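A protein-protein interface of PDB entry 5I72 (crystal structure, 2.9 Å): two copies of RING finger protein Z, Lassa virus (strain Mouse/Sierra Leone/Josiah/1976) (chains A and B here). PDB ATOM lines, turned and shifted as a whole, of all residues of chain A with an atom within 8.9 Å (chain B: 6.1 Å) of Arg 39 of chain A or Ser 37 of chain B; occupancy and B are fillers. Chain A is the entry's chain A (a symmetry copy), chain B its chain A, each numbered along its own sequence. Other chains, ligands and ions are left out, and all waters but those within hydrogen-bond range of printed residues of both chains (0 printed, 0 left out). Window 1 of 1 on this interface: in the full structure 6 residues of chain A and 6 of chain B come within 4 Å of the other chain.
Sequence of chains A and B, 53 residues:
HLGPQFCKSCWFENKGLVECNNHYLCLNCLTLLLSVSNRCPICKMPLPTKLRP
Of the 22 printed residues of chain A, 6 touch a printed residue of chain B. Printed residues of chain A that touch a printed residue of chain B: Val 36, Ser 37, Asn 38, Arg 39, Pro 41 and Lys 44. Hydrophobic or aromatic side chains of chain A that line the printed part of chain B: Pro 41. Among the printed residues, no Asp or Glu carboxylate lies within 4 Å of a Lys or Arg side-chain nitrogen of the other chain.
Among the printed residues, pairs that only touch across the chains: Lys 44 of chain A with Pro 41 of chain B, Pro 41 of chain A with Arg 39 of chain B, Arg 39 of chain A with Pro 41 of chain B, Ser 37 of chain A with Arg 39 of chain B, Arg 39 of chain A with Ser 37 of chain B and Ser 37 of chain A with Ser 37 of chain B.
Leu 25 of chain A touches none of the printed residues of chain B. Leu 34 of chain A touches none of the printed residues of chain B. Printed residues of chain B within 4 Å of Val 36 of chain A: Asn 38. Of the printed residues of chain B, Ser 37 of chain A touches Ser 37, Asn 38 and Arg 39. Arg 39 of chain A touches three residues of chain B. Of the printed residues of chain B, Pro 41 of chain A touches Arg 39. Of chain A, only Asn 38 (3.2 Å) comes within 4 Å of Val 36 of chain B. Ser 37 of chain B touches just these residues of chain A: Ser 37, Asn 38 and Arg 39. Of the printed residues of chain A, Asn 38 of chain B touches Val 36, Ser 37 and Asn 38. The nearest residue of chain A that does not touch Ser 37 of chain B is Cys 40 of chain A (6.7 Å). The nearest printed residue of chain B that does not touch Asn 38 of chain A is Arg 39 of chain B (5.1 Å).
Ser 37 of chain A touches Asn 38 of chain B, and with the chains exchanged Asn 38 of chain A touches Ser 37 of chain B. Asn 38 of chain B touches its own counterpart, Asn 38 of chain A. Arg 39 of chain A touches its own counterpart, Arg 39 of chain B. Arg 39 of chain A touches Pro 41 of chain B, and with the chains exchanged Pro 41 of chain A touches Arg 39 of chain B. Positions printed for both chains: 32, 33, 34, 35, 36, 37, 38, 39, 40, 41 and 47.
OD1 of Asn 38 of chain A is in hydrogen-bond range of OG of Ser 37 of chain B (2.6 Å). The backbone carbonyl oxygen of Arg 39 of chain B lies within hydrogen-bond range of the guanidinium group of Arg 39 of chain A (2.5 Å). The backbone carbonyl oxygen (O) of Val 36 of chain B lies within hydrogen-bond range of the side-chain amide nitrogen (ND2) of Asn 38 of chain A, at 3.2 Å. OD1 of Asn 38 of chain B is in hydrogen-bond range of OG of Ser 37 of chain A (2.6 Å). The backbone carbonyl oxygen of Val 36 of chain A sits at hydrogen-bond distance from the side-chain amide nitrogen of Asn 38 of chain B (3.2 Å). OD1 of Asn 38 of chain A lies close to OD1 of Asn 38 of chain B, 2.9 Å away.
OG of Ser 37 of chain A is in hydrogen-bond range of N of Arg 39 of chain A, 3.2 Å away. NE of Arg 39 of chain A is in hydrogen-bond range of O of Lys 44 of chain A (3.0 Å). OG of Ser 37 of chain B is in hydrogen-bond range of OD1 of Asn 38 of chain B, at 3.3 Å. The side-chain amide oxygen of Asn 38 of chain A lies within hydrogen-bond range of the side-chain hydroxyl of Ser 37 of chain A. OG of Ser 37 of chain B is in hydrogen-bond range of N of Arg 39 of chain B (3.2 Å). N of Leu 47 of chain A sits at hydrogen-bond distance from O of Asn 38 of chain A (2.9 Å).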
ATOM      1  N   CYS A  20       2.604  10.805   2.076  1.00  0.00           N
ATOM      2  CA  CYS A  20       1.460   9.930   2.281  1.00  0.00           C
ATOM      3  C   CYS A  20       0.232  10.801   2.050  1.00  0.00           C
ATOM      4  O   CYS A  20       0.372  11.958   1.652  1.00  0.00           O
ATOM      5  CB  CYS A  20       1.469   9.297   3.674  1.00  0.00           C
ATOM      6  SG  CYS A  20       0.495   7.769   3.824  1.00  0.00           S
ATOM      7  N   ASN A  21      -0.960  10.280   2.300  1.00  0.00           N
ATOM      8  CA  ASN A  21      -2.155  10.946   1.789  1.00  0.00           C
ATOM      9  C   ASN A  21      -2.442  12.317   2.416  1.00  0.00           C
ATOM     10  O   ASN A  21      -2.742  13.268   1.694  1.00  0.00           O
ATOM     11  CB  ASN A  21      -3.357  10.020   1.946  1.00  0.00           C
ATOM     12  CG  ASN A  21      -3.180   8.720   1.186  1.00  0.00           C
ATOM     13  OD1 ASN A  21      -3.505   8.634   0.001  1.00  0.00           O
ATOM     14  ND2 ASN A  21      -2.637   7.708   1.856  1.00  0.00           N
ATOM     15  N   HIS A  23      -0.276  13.394   5.233  1.00  0.00           N
ATOM     16  CA  HIS A  23       0.846  13.543   6.144  1.00  0.00           C
ATOM     17  C   HIS A  23       2.112  13.049   5.456  1.00  0.00           C
ATOM     18  O   HIS A  23       2.081  12.669   4.283  1.00  0.00           O
ATOM     19  CB  HIS A  23       0.608  12.761   7.433  1.00  0.00           C
ATOM     20  CG  HIS A  23       0.549  11.278   7.239  1.00  0.00           C
ATOM     21  ND1 HIS A  23       1.612  10.448   7.521  1.00  0.00           N
ATOM     22  CD2 HIS A  23      -0.446  10.477   6.786  1.00  0.00           C
ATOM     23  CE1 HIS A  23       1.277   9.198   7.252  1.00  0.00           C
ATOM     24  NE2 HIS A  23       0.034   9.188   6.804  1.00  0.00           N
ATOM     25  N   LEU A  25       5.883  10.610   5.590  1.00  0.00           N
ATOM     26  CA  LEU A  25       6.526   9.414   6.118  1.00  0.00           C
ATOM     27  C   LEU A  25       7.977   9.347   5.657  1.00  0.00           C
ATOM     28  O   LEU A  25       8.268   9.534   4.475  1.00  0.00           O
ATOM     29  CB  LEU A  25       5.783   8.150   5.679  1.00  0.00           C
ATOM     30  CG  LEU A  25       4.503   7.763   6.419  1.00  0.00           C
ATOM     31  CD1 LEU A  25       3.878   6.526   5.788  1.00  0.00           C
ATOM     32  CD2 LEU A  25       4.799   7.524   7.887  1.00  0.00           C
ATOM     33  N   LEU A  30       8.067   4.107   6.285  1.00  0.00           N
ATOM     34  CA  LEU A  30       7.254   3.657   5.157  1.00  0.00           C
ATOM     35  C   LEU A  30       7.514   2.188   4.840  1.00  0.00           C
ATOM     36  O   LEU A  30       6.585   1.431   4.553  1.00  0.00           O
ATOM     37  CB  LEU A  30       7.533   4.516   3.922  1.00  0.00           C
ATOM     38  CG  LEU A  30       6.855   4.097   2.616  1.00  0.00           C
ATOM     39  CD1 LEU A  30       5.359   3.884   2.816  1.00  0.00           C
ATOM     40  CD2 LEU A  30       7.112   5.135   1.536  1.00  0.00           C
ATOM     41  N   LEU A  32       8.713  -0.213   6.905  1.00  0.00           N
ATOM     42  CA  LEU A  32       8.209  -1.058   7.978  1.00  0.00           C
ATOM     43  C   LEU A  32       6.686  -1.170   7.913  1.00  0.00           C
ATOM     44  O   LEU A  32       6.120  -2.227   8.195  1.00  0.00           O
ATOM     45  CB  LEU A  32       8.656  -0.513   9.337  1.00  0.00           C
ATOM     46  CG  LEU A  32       8.264  -1.305  10.584  1.00  0.00           C
ATOM     47  CD1 LEU A  32       8.650  -2.767  10.432  1.00  0.00           C
ATOM     48  CD2 LEU A  32       8.931  -0.701  11.811  1.00  0.00           C
ATOM     49  N   LEU A  33       6.026  -0.078   7.536  1.00  0.00           N
ATOM     50  CA  LEU A  33       4.574  -0.079   7.400  1.00  0.00           C
ATOM     51  C   LEU A  33       4.129  -0.907   6.193  1.00  0.00           C
ATOM     52  O   LEU A  33       3.105  -1.581   6.243  1.00  0.00           O
ATOM     53  CB  LEU A  33       4.035   1.348   7.280  1.00  0.00           C
ATOM     54  CG  LEU A  33       4.196   2.279   8.485  1.00  0.00           C
ATOM     55  CD1 LEU A  33       3.683   3.668   8.141  1.00  0.00           C
ATOM     56  CD2 LEU A  33       3.489   1.734   9.721  1.00  0.00           C
ATOM     57  N   LEU A  34       4.880  -0.828   5.098  1.00  0.00           N
ATOM     58  CA  LEU A  34       4.566  -1.628   3.917  1.00  0.00           C
ATOM     59  C   LEU A  34       4.825  -3.104   4.187  1.00  0.00           C
ATOM     60  O   LEU A  34       4.113  -3.977   3.686  1.00  0.00           O
ATOM     61  CB  LEU A  34       5.381  -1.160   2.711  1.00  0.00           C
ATOM     62  CG  LEU A  34       4.811   0.048   1.971  1.00  0.00           C
ATOM     63  CD1 LEU A  34       5.823   0.612   0.990  1.00  0.00           C
ATOM     64  CD2 LEU A  34       3.525  -0.344   1.260  1.00  0.00           C
ATOM     65  N   SER A  35       5.854  -3.362   4.989  1.00  0.00           N
ATOM     66  CA  SER A  35       6.164  -4.699   5.472  1.00  0.00           C
ATOM     67  C   SER A  35       4.964  -5.394   6.108  1.00  0.00           C
ATOM     68  O   SER A  35       4.832  -6.616   6.037  1.00  0.00           O
ATOM     69  CB  SER A  35       7.317  -4.627   6.481  1.00  0.00           C
ATOM     70  OG  SER A  35       7.198  -5.621   7.484  1.00  0.00           O
ATOM     71  N   VAL A  36       4.082  -4.610   6.717  1.00  0.00           N
ATOM     72  CA  VAL A  36       3.017  -5.174   7.531  1.00  0.00           C
ATOM     73  C   VAL A  36       1.633  -5.139   6.858  1.00  0.00           C
ATOM     74  O   VAL A  36       0.806  -6.021   7.106  1.00  0.00           O
ATOM     75  CB  VAL A  36       2.970  -4.469   8.906  1.00  0.00           C
ATOM     76  CG1 VAL A  36       2.411  -3.057   8.805  1.00  0.00           C
ATOM     77  CG2 VAL A  36       2.199  -5.294   9.882  1.00  0.00           C
ATOM     78  N   SER A  37       1.380  -4.138   6.015  1.00  0.00           N
ATOM     79  CA  SER A  37       0.097  -4.022   5.311  1.00  0.00           C
ATOM     80  C   SER A  37       0.139  -2.936   4.236  1.00  0.00           C
ATOM     81  O   SER A  37       1.033  -2.093   4.233  1.00  0.00           O
ATOM     82  CB  SER A  37      -1.040  -3.728   6.294  1.00  0.00           C
ATOM     83  OG  SER A  37      -2.254  -3.469   5.610  1.00  0.00           O
ATOM     84  N   ASN A  38      -0.831  -2.958   3.327  1.00  0.00           N
ATOM     85  CA  ASN A  38      -0.924  -1.928   2.294  1.00  0.00           C
ATOM     86  C   ASN A  38      -1.658  -0.685   2.782  1.00  0.00           C
ATOM     87  O   ASN A  38      -1.682   0.337   2.094  1.00  0.00           O
ATOM     88  CB  ASN A  38      -1.626  -2.473   1.048  1.00  0.00           C
ATOM     89  CG  ASN A  38      -2.893  -3.233   1.380  1.00  0.00           C
ATOM     90  OD1 ASN A  38      -3.003  -3.838   2.446  1.00  0.00           O
ATOM     91  ND2 ASN A  38      -3.862  -3.203   0.468  1.00  0.00           N
ATOM     92  N   ARG A  39      -2.255  -0.776   3.967  1.00  0.00           N
ATOM     93  CA  ARG A  39      -3.048   0.326   4.509  1.00  0.00           C
ATOM     94  C   ARG A  39      -2.336   1.022   5.668  1.00  0.00           C
ATOM     95  O   ARG A  39      -1.843   0.376   6.592  1.00  0.00           O
ATOM     96  CB  ARG A  39      -4.416  -0.185   4.958  1.00  0.00           C
ATOM     97  CG  ARG A  39      -5.240   0.816   5.744  1.00  0.00           C
ATOM     98  CD  ARG A  39      -6.656   0.300   5.921  1.00  0.00           C
ATOM     99  NE  ARG A  39      -7.517   0.774   4.845  1.00  0.00           N
ATOM    100  CZ  ARG A  39      -8.524   0.080   4.330  1.00  0.00           C
ATOM    101  NH1 ARG A  39      -8.811  -1.129   4.792  1.00  0.00           N
ATOM    102  NH2 ARG A  39      -9.245   0.598   3.348  1.00  0.00           N
ATOM    103  N   CYS A  40      -2.298   2.348   5.611  1.00  0.00           N
ATOM    104  CA  CYS A  40      -1.591   3.150   6.603  1.00  0.00           C
ATOM    105  C   CYS A  40      -2.375   3.223   7.911  1.00  0.00           C
ATOM    106  O   CYS A  40      -3.571   3.504   7.906  1.00  0.00           O
ATOM    107  CB  CYS A  40      -1.337   4.554   6.041  1.00  0.00           C
ATOM    108  SG  CYS A  40      -0.511   5.704   7.147  1.00  0.00           S
ATOM    109  N   PRO A  41      -1.701   2.971   9.043  1.00  0.00           N
ATOM    110  CA  PRO A  41      -2.376   2.979  10.345  1.00  0.00           C
ATOM    111  C   PRO A  41      -2.597   4.390  10.876  1.00  0.00           C
ATOM    112  O   PRO A  41      -3.311   4.580  11.856  1.00  0.00           O
ATOM    113  CB  PRO A  41      -1.407   2.209  11.241  1.00  0.00           C
ATOM    114  CG  PRO A  41      -0.064   2.526  10.666  1.00  0.00           C
ATOM    115  CD  PRO A  41      -0.264   2.665   9.170  1.00  0.00           C
ATOM    116  N   ILE A  42      -1.982   5.374  10.232  1.00  0.00           N
ATOM    117  CA  ILE A  42      -2.064   6.751  10.696  1.00  0.00           C
ATOM    118  C   ILE A  42      -3.253   7.484  10.079  1.00  0.00           C
ATOM    119  O   ILE A  42      -3.951   8.235  10.760  1.00  0.00           O
ATOM    120  CB  ILE A  42      -0.773   7.518  10.368  1.00  0.00           C
ATOM    121  CG1 ILE A  42       0.409   6.913  11.124  1.00  0.00           C
ATOM    122  CG2 ILE A  42      -0.931   8.996  10.686  1.00  0.00           C
ATOM    123  CD1 ILE A  42       1.753   7.290  10.542  1.00  0.00           C
ATOM    124  N   CYS A  43      -3.487   7.253   8.791  1.00  0.00           N
ATOM    125  CA  CYS A  43      -4.526   7.981   8.068  1.00  0.00           C
ATOM    126  C   CYS A  43      -5.574   7.058   7.443  1.00  0.00           C
ATOM    127  O   CYS A  43      -6.501   7.532   6.784  1.00  0.00           O
ATOM    128  CB  CYS A  43      -3.894   8.862   6.984  1.00  0.00           C
ATOM    129  SG  CYS A  43      -3.180   7.959   5.587  1.00  0.00           S
ATOM    130  N   LYS A  44      -5.401   5.751   7.635  1.00  0.00           N
ATOM    131  CA  LYS A  44      -6.377   4.735   7.221  1.00  0.00           C
ATOM    132  C   LYS A  44      -6.478   4.569   5.695  1.00  0.00           C
ATOM    133  O   LYS A  44      -7.226   3.723   5.206  1.00  0.00           O
ATOM    134  CB  LYS A  44      -7.752   5.055   7.827  1.00  0.00           C
ATOM    135  CG  LYS A  44      -7.786   4.897   9.350  1.00  0.00           C
ATOM    136  CD  LYS A  44      -8.785   5.831  10.020  1.00  0.00           C
ATOM    137  CE  LYS A  44     -10.182   5.672   9.453  1.00  0.00           C
ATOM    138  NZ  LYS A  44     -11.178   6.518  10.165  1.00  0.00           N
ATOM    139  N   MET A  45      -5.706   5.356   4.950  1.00  0.00           N
ATOM    140  CA  MET A  45      -5.710   5.287   3.487  1.00  0.00           C
ATOM    141  C   MET A  45      -4.520   4.475   2.949  1.00  0.00           C
ATOM    142  O   MET A  45      -3.627   4.112   3.715  1.00  0.00           O
ATOM    143  CB  MET A  45      -5.716   6.708   2.917  1.00  0.00           C
ATOM    144  CG  MET A  45      -7.076   7.376   3.021  1.00  0.00           C
ATOM    145  SD  MET A  45      -7.017   9.153   2.760  1.00  0.00           S
ATOM    146  CE  MET A  45      -6.283   9.695   4.298  1.00  0.00           C
ATOM    147  N   PRO A  46      -4.506   4.170   1.634  1.00  0.00           N
ATOM    148  CA  PRO A  46      -3.422   3.302   1.155  1.00  0.00           C
ATOM    149  C   PRO A  46      -2.042   3.941   1.242  1.00  0.00           C
ATOM    150  O   PRO A  46      -1.891   5.147   1.031  1.00  0.00           O
ATOM    151  CB  PRO A  46      -3.802   3.036  -0.311  1.00  0.00           C
ATOM    152  CG  PRO A  46      -4.738   4.125  -0.674  1.00  0.00           C
ATOM    153  CD  PRO A  46      -5.509   4.399   0.579  1.00  0.00           C
ATOM    154  N   LEU A  47      -1.051   3.121   1.573  1.00  0.00           N
ATOM    155  CA  LEU A  47       0.337   3.562   1.640  1.00  0.00           C
ATOM    156  C   LEU A  47       0.897   3.856   0.255  1.00  0.00           C
ATOM    157  O   LEU A  47       0.456   3.270  -0.735  1.00  0.00           O
ATOM    158  CB  LEU A  47       1.203   2.508   2.336  1.00  0.00           C
ATOM    159  CG  LEU A  47       1.104   2.458   3.861  1.00  0.00           C
ATOM    160  CD1 LEU A  47       1.538   1.100   4.389  1.00  0.00           C
ATOM    161  CD2 LEU A  47       1.944   3.564   4.473  1.00  0.00           C
ATOM    162  N   PRO A  48       1.871   4.773   0.182  1.00  0.00           N
ATOM    163  CA  PRO A  48       2.571   5.054  -1.074  1.00  0.00           C
ATOM    164  C   PRO A  48       3.393   3.846  -1.512  1.00  0.00           C
ATOM    165  O   PRO A  48       4.147   3.288  -0.712  1.00  0.00           O
ATOM    166  CB  PRO A  48       3.470   6.249  -0.728  1.00  0.00           C
ATOM    167  CG  PRO A  48       2.888   6.831   0.515  1.00  0.00           C
ATOM    168  CD  PRO A  48       2.312   5.670   1.263  1.00  0.00           C
ATOM    169  N   LEU B  32     -15.714  -7.680   1.524  1.00  0.00           N
ATOM    170  CA  LEU B  32     -15.363  -6.521   0.714  1.00  0.00           C
ATOM    171  C   LEU B  32     -14.133  -5.813   1.281  1.00  0.00           C
ATOM    172  O   LEU B  32     -13.295  -5.312   0.532  1.00  0.00           O
ATOM    173  CB  LEU B  32     -16.550  -5.559   0.624  1.00  0.00           C
ATOM    174  CG  LEU B  32     -16.385  -4.306  -0.235  1.00  0.00           C
ATOM    175  CD1 LEU B  32     -15.874  -4.670  -1.620  1.00  0.00           C
ATOM    176  CD2 LEU B  32     -17.711  -3.567  -0.333  1.00  0.00           C
ATOM    177  N   LEU B  33     -14.027  -5.777   2.607  1.00  0.00           N
ATOM    178  CA  LEU B  33     -12.875  -5.164   3.259  1.00  0.00           C
ATOM    179  C   LEU B  33     -11.612  -6.003   3.062  1.00  0.00           C
ATOM    180  O   LEU B  33     -10.523  -5.461   2.901  1.00  0.00           O
ATOM    181  CB  LEU B  33     -13.138  -4.958   4.752  1.00  0.00           C
ATOM    182  CG  LEU B  33     -14.239  -3.974   5.159  1.00  0.00           C
ATOM    183  CD1 LEU B  33     -14.407  -3.976   6.669  1.00  0.00           C
ATOM    184  CD2 LEU B  33     -13.957  -2.565   4.649  1.00  0.00           C
ATOM    185  N   LEU B  34     -11.752  -7.324   3.112  1.00  0.00           N
ATOM    186  CA  LEU B  34     -10.613  -8.207   2.878  1.00  0.00           C
ATOM    187  C   LEU B  34     -10.178  -8.143   1.421  1.00  0.00           C
ATOM    188  O   LEU B  34      -8.990  -8.240   1.105  1.00  0.00           O
ATOM    189  CB  LEU B  34     -10.951  -9.647   3.267  1.00  0.00           C
ATOM    190  CG  LEU B  34     -10.817  -9.966   4.755  1.00  0.00           C
ATOM    191  CD1 LEU B  34     -11.447 -11.309   5.081  1.00  0.00           C
ATOM    192  CD2 LEU B  34      -9.349  -9.943   5.155  1.00  0.00           C
ATOM    193  N   SER B  35     -11.162  -7.976   0.543  1.00  0.00           N
ATOM    194  CA  SER B  35     -10.927  -7.751  -0.877  1.00  0.00           C
ATOM    195  C   SER B  35      -9.943  -6.615  -1.142  1.00  0.00           C
ATOM    196  O   SER B  35      -9.198  -6.642  -2.121  1.00  0.00           O
ATOM    197  CB  SER B  35     -12.259  -7.458  -1.579  1.00  0.00           C
ATOM    198  OG  SER B  35     -12.093  -6.559  -2.661  1.00  0.00           O
ATOM    199  N   VAL B  36      -9.933  -5.624  -0.257  1.00  0.00           N
ATOM    200  CA  VAL B  36      -9.193  -4.400  -0.515  1.00  0.00           C
ATOM    201  C   VAL B  36      -7.883  -4.282   0.285  1.00  0.00           C
ATOM    202  O   VAL B  36      -6.921  -3.675  -0.193  1.00  0.00           O
ATOM    203  CB  VAL B  36     -10.096  -3.170  -0.263  1.00  0.00           C
ATOM    204  CG1 VAL B  36     -10.343  -2.939   1.221  1.00  0.00           C
ATOM    205  CG2 VAL B  36      -9.513  -1.961  -0.916  1.00  0.00           C
ATOM    206  N   SER B  37      -7.840  -4.856   1.487  1.00  0.00           N
ATOM    207  CA  SER B  37      -6.633  -4.815   2.324  1.00  0.00           C
ATOM    208  C   SER B  37      -6.757  -5.736   3.538  1.00  0.00           C
ATOM    209  O   SER B  37      -7.854  -6.166   3.888  1.00  0.00           O
ATOM    210  CB  SER B  37      -6.344  -3.386   2.791  1.00  0.00           C
ATOM    211  OG  SER B  37      -5.270  -3.358   3.716  1.00  0.00           O
ATOM    212  N   ASN B  38      -5.630  -6.032   4.179  1.00  0.00           N
ATOM    213  CA  ASN B  38      -5.641  -6.849   5.391  1.00  0.00           C
ATOM    214  C   ASN B  38      -5.923  -6.026   6.641  1.00  0.00           C
ATOM    215  O   ASN B  38      -6.128  -6.581   7.722  1.00  0.00           O
ATOM    216  CB  ASN B  38      -4.311  -7.586   5.559  1.00  0.00           C
ATOM    217  CG  ASN B  38      -3.115  -6.681   5.349  1.00  0.00           C
ATOM    218  OD1 ASN B  38      -3.180  -5.721   4.581  1.00  0.00           O
ATOM    219  ND2 ASN B  38      -2.014  -6.979   6.035  1.00  0.00           N
ATOM    220  N   ARG B  39      -5.930  -4.705   6.492  1.00  0.00           N
ATOM    221  CA  ARG B  39      -6.118  -3.808   7.631  1.00  0.00           C
ATOM    222  C   ARG B  39      -7.496  -3.147   7.613  1.00  0.00           C
ATOM    223  O   ARG B  39      -7.934  -2.616   6.593  1.00  0.00           O
ATOM    224  CB  ARG B  39      -5.021  -2.744   7.647  1.00  0.00           C
ATOM    225  CG  ARG B  39      -5.239  -1.624   8.645  1.00  0.00           C
ATOM    226  CD  ARG B  39      -3.988  -0.771   8.751  1.00  0.00           C
ATOM    227  NE  ARG B  39      -3.123  -1.254   9.820  1.00  0.00           N
ATOM    228  CZ  ARG B  39      -1.797  -1.210   9.789  1.00  0.00           C
ATOM    229  NH1 ARG B  39      -1.167  -0.698   8.740  1.00  0.00           N
ATOM    230  NH2 ARG B  39      -1.099  -1.681  10.810  1.00  0.00           N
ATOM    231  N   CYS B  40      -8.169  -3.182   8.757  1.00  0.00           N
ATOM    232  CA  CYS B  40      -9.525  -2.661   8.878  1.00  0.00           C
ATOM    233  C   CYS B  40      -9.527  -1.134   8.916  1.00  0.00           C
ATOM    234  O   CYS B  40      -8.766  -0.528   9.667  1.00  0.00           O
ATOM    235  CB  CYS B  40     -10.185  -3.236  10.136  1.00  0.00           C
ATOM    236  SG  CYS B  40     -11.856  -2.667  10.477  1.00  0.00           S
ATOM    237  N   PRO B  41     -10.387  -0.503   8.103  1.00  0.00           N
ATOM    238  CA  PRO B  41     -10.435   0.962   8.040  1.00  0.00           C
ATOM    239  C   PRO B  41     -11.205   1.569   9.206  1.00  0.00           C
ATOM    240  O   PRO B  41     -11.178   2.780   9.405  1.00  0.00           O
ATOM    241  CB  PRO B  41     -11.155   1.227   6.719  1.00  0.00           C
ATOM    242  CG  PRO B  41     -12.083   0.063   6.580  1.00  0.00           C
ATOM    243  CD  PRO B  41     -11.368  -1.125   7.195  1.00  0.00           C
ATOM    244  N   LEU B  47      -7.785  -7.276  10.001  1.00  0.00           N
ATOM    245  CA  LEU B  47      -9.081  -7.906   9.775  1.00  0.00           C
ATOM    246  C   LEU B  47      -9.063  -9.376  10.170  1.00  0.00           C
ATOM    247  O   LEU B  47      -8.016 -10.024  10.122  1.00  0.00           O
ATOM    248  CB  LEU B  47      -9.496  -7.769   8.308  1.00  0.00           C
ATOM    249  CG  LEU B  47     -10.043  -6.404   7.889  1.00  0.00           C
ATOM    250  CD1 LEU B  47      -9.909  -6.202   6.388  1.00  0.00           C
ATOM    251  CD2 LEU B  47     -11.491  -6.269   8.320  1.00  0.00           C
